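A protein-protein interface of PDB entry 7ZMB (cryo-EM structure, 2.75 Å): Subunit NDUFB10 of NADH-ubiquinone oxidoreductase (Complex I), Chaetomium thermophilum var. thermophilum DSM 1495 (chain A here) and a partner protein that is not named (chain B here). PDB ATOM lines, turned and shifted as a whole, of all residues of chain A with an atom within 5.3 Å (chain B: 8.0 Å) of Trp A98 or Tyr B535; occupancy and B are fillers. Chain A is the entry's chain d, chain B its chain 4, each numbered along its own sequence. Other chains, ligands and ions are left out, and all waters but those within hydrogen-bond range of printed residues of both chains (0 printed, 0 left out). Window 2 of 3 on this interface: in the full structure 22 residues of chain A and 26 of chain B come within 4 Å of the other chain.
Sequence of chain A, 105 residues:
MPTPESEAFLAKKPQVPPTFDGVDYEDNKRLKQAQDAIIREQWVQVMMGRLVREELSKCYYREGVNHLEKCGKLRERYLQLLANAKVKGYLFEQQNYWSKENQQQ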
ATOM      1  N   PHE A  92      -9.992  25.237   3.976  1.00  0.00           N
ATOM      2  CA  PHE A  92      -9.953  24.867   5.384  1.00  0.00           C
ATOM      3  C   PHE A  92      -9.846  23.359   5.553  1.00  0.00           C
ATOM      4  O   PHE A  92      -9.164  22.879   6.463  1.00  0.00           O
ATOM      5  CB  PHE A  92     -11.179  25.408   6.113  1.00  0.00           C
ATOM      6  CG  PHE A  92     -10.966  25.573   7.577  1.00  0.00           C
ATOM      7  CD1 PHE A  92     -11.200  24.526   8.443  1.00  0.00           C
ATOM      8  CD2 PHE A  92     -10.508  26.767   8.090  1.00  0.00           C
ATOM      9  CE1 PHE A  92     -10.992  24.670   9.784  1.00  0.00           C
ATOM     10  CE2 PHE A  92     -10.290  26.913   9.435  1.00  0.00           C
ATOM     11  CZ  PHE A  92     -10.534  25.861  10.284  1.00  0.00           C
ATOM     12  N   GLU A  93     -10.527  22.598   4.692  1.00  0.00           N
ATOM     13  CA  GLU A  93     -10.361  21.148   4.673  1.00  0.00           C
ATOM     14  C   GLU A  93      -8.923  20.762   4.358  1.00  0.00           C
ATOM     15  O   GLU A  93      -8.342  19.899   5.024  1.00  0.00           O
ATOM     16  CB  GLU A  93     -11.294  20.530   3.633  1.00  0.00           C
ATOM     17  CG  GLU A  93     -12.771  20.524   3.978  1.00  0.00           C
ATOM     18  CD  GLU A  93     -13.147  19.402   4.913  1.00  0.00           C
ATOM     19  OE1 GLU A  93     -12.556  18.314   4.795  1.00  0.00           O
ATOM     20  OE2 GLU A  93     -14.041  19.600   5.751  1.00  0.00           O
ATOM     21  N   ASN A  96      -6.470  21.774   7.462  1.00  0.00           N
ATOM     22  CA  ASN A  96      -6.741  21.299   8.810  1.00  0.00           C
ATOM     23  C   ASN A  96      -7.379  19.923   8.749  1.00  0.00           C
ATOM     24  O   ASN A  96      -8.205  19.644   7.879  1.00  0.00           O
ATOM     25  CB  ASN A  96      -7.649  22.263   9.580  1.00  0.00           C
ATOM     26  CG  ASN A  96      -7.230  23.699   9.419  1.00  0.00           C
ATOM     27  OD1 ASN A  96      -6.213  24.122   9.955  1.00  0.00           O
ATOM     28  ND2 ASN A  96      -8.000  24.454   8.655  1.00  0.00           N
ATOM     29  N   TYR A  97      -6.972  19.057   9.670  1.00  0.00           N
ATOM     30  CA  TYR A  97      -7.568  17.736   9.811  1.00  0.00           C
ATOM     31  C   TYR A  97      -8.214  17.653  11.186  1.00  0.00           C
ATOM     32  O   TYR A  97      -7.629  18.083  12.183  1.00  0.00           O
ATOM     33  CB  TYR A  97      -6.541  16.622   9.593  1.00  0.00           C
ATOM     34  CG  TYR A  97      -5.408  16.568  10.591  1.00  0.00           C
ATOM     35  CD1 TYR A  97      -4.230  17.269  10.374  1.00  0.00           C
ATOM     36  CD2 TYR A  97      -5.514  15.809  11.748  1.00  0.00           C
ATOM     37  CE1 TYR A  97      -3.190  17.212  11.278  1.00  0.00           C
ATOM     38  CE2 TYR A  97      -4.482  15.755  12.662  1.00  0.00           C
ATOM     39  CZ  TYR A  97      -3.324  16.458  12.423  1.00  0.00           C
ATOM     40  OH  TYR A  97      -2.292  16.404  13.331  1.00  0.00           O
ATOM     41  N   TRP A  98      -9.434  17.116  11.227  1.00  0.00           N
ATOM     42  CA  TRP A  98     -10.196  17.099  12.469  1.00  0.00           C
ATOM     43  C   TRP A  98     -10.182  15.714  13.106  1.00  0.00           C
ATOM     44  O   TRP A  98     -10.098  15.591  14.334  1.00  0.00           O
ATOM     45  CB  TRP A  98     -11.617  17.578  12.189  1.00  0.00           C
ATOM     46  CG  TRP A  98     -12.629  17.157  13.185  1.00  0.00           C
ATOM     47  CD1 TRP A  98     -12.660  17.471  14.511  1.00  0.00           C
ATOM     48  CD2 TRP A  98     -13.785  16.355  12.935  1.00  0.00           C
ATOM     49  NE1 TRP A  98     -13.761  16.904  15.105  1.00  0.00           N
ATOM     50  CE2 TRP A  98     -14.467  16.214  14.158  1.00  0.00           C
ATOM     51  CE3 TRP A  98     -14.304  15.740  11.797  1.00  0.00           C
ATOM     52  CZ2 TRP A  98     -15.645  15.482  14.272  1.00  0.00           C
ATOM     53  CZ3 TRP A  98     -15.470  15.013  11.912  1.00  0.00           C
ATOM     54  CH2 TRP A  98     -16.128  14.888  13.141  1.00  0.00           C
ATOM     55  N   SER A  99     -10.259  14.663  12.286  1.00  0.00           N
ATOM     56  CA  SER A  99     -10.045  13.283  12.728  1.00  0.00           C
ATOM     57  C   SER A  99     -10.999  12.880  13.849  1.00  0.00           C
ATOM     58  O   SER A  99     -10.613  12.187  14.793  1.00  0.00           O
ATOM     59  CB  SER A  99      -8.590  13.065  13.156  1.00  0.00           C
ATOM     60  OG  SER A  99      -7.691  13.547  12.173  1.00  0.00           O
ATOM     61  N   LYS A 100     -12.252  13.316  13.743  1.00  0.00           N
ATOM     62  CA  LYS A 100     -13.298  12.954  14.699  1.00  0.00           C
ATOM     63  C   LYS A 100     -12.910  13.284  16.138  1.00  0.00           C
ATOM     64  O   LYS A 100     -13.111  12.478  17.045  1.00  0.00           O
ATOM     65  CB  LYS A 100     -13.638  11.465  14.582  1.00  0.00           C
ATOM     66  N   ILE B 529     -15.605  26.337   6.959  1.00  0.00           N
ATOM     67  CA  ILE B 529     -16.319  25.034   6.853  1.00  0.00           C
ATOM     68  C   ILE B 529     -17.627  25.138   7.632  1.00  0.00           C
ATOM     69  O   ILE B 529     -17.716  25.999   8.514  1.00  0.00           O
ATOM     70  CB  ILE B 529     -15.450  23.890   7.413  1.00  0.00           C
ATOM     71  CG1 ILE B 529     -14.930  24.206   8.817  1.00  0.00           C
ATOM     72  CG2 ILE B 529     -14.325  23.529   6.457  1.00  0.00           C
ATOM     73  CD1 ILE B 529     -14.427  22.996   9.565  1.00  0.00           C
ATOM     74  N   GLU B 530     -18.596  24.286   7.303  1.00  0.00           N
ATOM     75  CA  GLU B 530     -19.860  24.253   8.070  1.00  0.00           C
ATOM     76  C   GLU B 530     -19.859  22.993   8.958  1.00  0.00           C
ATOM     77  O   GLU B 530     -19.335  21.964   8.493  1.00  0.00           O
ATOM     78  CB  GLU B 530     -21.055  24.244   7.113  1.00  0.00           C
ATOM     79  CG  GLU B 530     -21.128  25.475   6.229  1.00  0.00           C
ATOM     80  CD  GLU B 530     -21.510  26.747   6.964  1.00  0.00           C
ATOM     81  OE1 GLU B 530     -22.474  26.701   7.754  1.00  0.00           O
ATOM     82  OE2 GLU B 530     -20.839  27.776   6.755  1.00  0.00           O
ATOM     83  N   PRO B 531     -20.415  23.004  10.197  1.00  0.00           N
ATOM     84  CA  PRO B 531     -20.356  21.835  11.090  1.00  0.00           C
ATOM     85  C   PRO B 531     -20.955  20.573  10.502  1.00  0.00           C
ATOM     86  O   PRO B 531     -20.511  19.473  10.851  1.00  0.00           O
ATOM     87  CB  PRO B 531     -21.135  22.303  12.325  1.00  0.00           C
ATOM     88  CG  PRO B 531     -21.134  23.791  12.238  1.00  0.00           C
ATOM     89  CD  PRO B 531     -21.195  24.101  10.787  1.00  0.00           C
ATOM     90  N   ASN B 532     -21.952  20.686   9.626  1.00  0.00           N
ATOM     91  CA  ASN B 532     -22.650  19.522   9.096  1.00  0.00           C
ATOM     92  C   ASN B 532     -22.291  19.218   7.648  1.00  0.00           C
ATOM     93  O   ASN B 532     -22.909  18.337   7.041  1.00  0.00           O
ATOM     94  CB  ASN B 532     -24.161  19.709   9.232  1.00  0.00           C
ATOM     95  CG  ASN B 532     -24.615  19.751  10.675  1.00  0.00           C
ATOM     96  OD1 ASN B 532     -24.235  18.902  11.481  1.00  0.00           O
ATOM     97  ND2 ASN B 532     -25.435  20.739  11.010  1.00  0.00           N
ATOM     98  N   ALA B 533     -21.308  19.916   7.076  1.00  0.00           N
ATOM     99  CA  ALA B 533     -20.915  19.647   5.698  1.00  0.00           C
ATOM    100  C   ALA B 533     -19.408  19.472   5.549  1.00  0.00           C
ATOM    101  O   ALA B 533     -18.918  19.330   4.423  1.00  0.00           O
ATOM    102  CB  ALA B 533     -21.397  20.762   4.765  1.00  0.00           C
ATOM    103  N   SER B 534     -18.662  19.470   6.648  1.00  0.00           N
ATOM    104  CA  SER B 534     -17.217  19.303   6.618  1.00  0.00           C
ATOM    105  C   SER B 534     -16.862  17.864   6.946  1.00  0.00           C
ATOM    106  O   SER B 534     -17.539  17.218   7.752  1.00  0.00           O
ATOM    107  CB  SER B 534     -16.532  20.242   7.609  1.00  0.00           C
ATOM    108  OG  SER B 534     -17.039  20.057   8.919  1.00  0.00           O
ATOM    109  N   TYR B 535     -15.804  17.367   6.311  1.00  0.00           N
ATOM    110  CA  TYR B 535     -15.271  16.033   6.583  1.00  0.00           C
ATOM    111  C   TYR B 535     -16.326  14.946   6.375  1.00  0.00           C
ATOM    112  O   TYR B 535     -16.530  14.076   7.225  1.00  0.00           O
ATOM    113  CB  TYR B 535     -14.689  15.961   7.994  1.00  0.00           C
ATOM    114  CG  TYR B 535     -13.776  17.105   8.330  1.00  0.00           C
ATOM    115  CD1 TYR B 535     -12.520  17.201   7.760  1.00  0.00           C
ATOM    116  CD2 TYR B 535     -14.166  18.084   9.216  1.00  0.00           C
ATOM    117  CE1 TYR B 535     -11.681  18.246   8.062  1.00  0.00           C
ATOM    118  CE2 TYR B 535     -13.333  19.131   9.524  1.00  0.00           C
ATOM    119  CZ  TYR B 535     -12.095  19.207   8.945  1.00  0.00           C
ATOM    120  OH  TYR B 535     -11.255  20.246   9.256  1.00  0.00           O
ATOM    121  N   LEU B 536     -17.004  15.003   5.233  1.00  0.00           N
ATOM    122  CA  LEU B 536     -17.942  13.949   4.877  1.00  0.00           C
ATOM    123  C   LEU B 536     -17.196  12.646   4.619  1.00  0.00           C
ATOM    124  O   LEU B 536     -16.147  12.630   3.972  1.00  0.00           O
ATOM    125  CB  LEU B 536     -18.748  14.346   3.642  1.00  0.00           C
ATOM    126  CG  LEU B 536     -19.584  15.621   3.760  1.00  0.00           C
ATOM    127  CD1 LEU B 536     -20.314  15.907   2.458  1.00  0.00           C
ATOM    128  CD2 LEU B 536     -20.568  15.506   4.911  1.00  0.00           C
ATOM    129  N   THR B 537     -17.741  11.549   5.135  1.00  0.00           N
ATOM    130  CA  THR B 537     -17.126  10.238   4.958  1.00  0.00           C
ATOM    131  C   THR B 537     -18.130   9.232   4.405  1.00  0.00           C
ATOM    132  O   THR B 537     -17.759   8.300   3.692  1.00  0.00           O
ATOM    133  CB  THR B 537     -16.545   9.701   6.279  1.00  0.00           C
ATOM    134  OG1 THR B 537     -17.568   9.684   7.283  1.00  0.00           O
ATOM    135  CG2 THR B 537     -15.393  10.572   6.750  1.00  0.00           C
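N of Tyr B535 sits at hydrogen-bond distance from OE2 of Glu A93 (2.9 Å).
O of Asn A96 lies within hydrogen-bond range of OH of Tyr B535 (3.4 Å).
The side-chain hydroxyl of Ser B534 sits at hydrogen-bond distance from the backbone carbonyl oxygen of Glu B530, 3.0 Å away.
The backbone carbonyl oxygen (O) of Phe A92 sits at hydrogen-bond distance from the side-chain amide nitrogen (ND2) of Asn A96, 2.9 Å away.
CB of Phe A92 touches CG2 of Ile B529, 3.7 Å away.
Glu A93 touches Ser B534.
CD2 of Tyr B535 touches CE3 of Trp A98, 3.5 Å away.
Hydrophobic or aromatic side chains of chain A that line the printed part of chain B: Phe A92 and Trp A98.
Of the 9 printed residues of chain B, 3 touch a printed residue of chain A.
Along chain B the printed residues that touch a printed residue of chain A span positions 529 to 535.
Among the printed residues, 5 pairs touch across the chains.
Among the printed residues, no Asp or Glu carboxylate lies within 4 Å of a Lys or Arg side-chain nitrogen of the other chain.
Trp A98 touches just one residue of chain B: Tyr B535.
No residue of chain B comes within 4 Å of Ser A99.
Of the printed residues of chain B, Phe A92 touches Ile B529 (3.7 Å).
Printed residues of chain B within 4 Å of Asn A96: Tyr B535.
Printed residues of chain A within 4 Å of Ile B529: Phe A92 (3.7 Å).
Printed residues of chain A within 4 Å of Ser B534: Glu A93.
Pro B531 touches none of the printed residues of chain A.
Thr B537 touches none of the printed residues of chain A.
The nearest residue of chain B that does not touch Trp A98 is Ser B534 (5.1 Å).
The nearest residue of chain A that does not touch Tyr B535 is Phe A92 (4.4 Å).
The nearest printed residue of chain A that does not touch Ile B529 is Glu A93 (4.002 Å).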
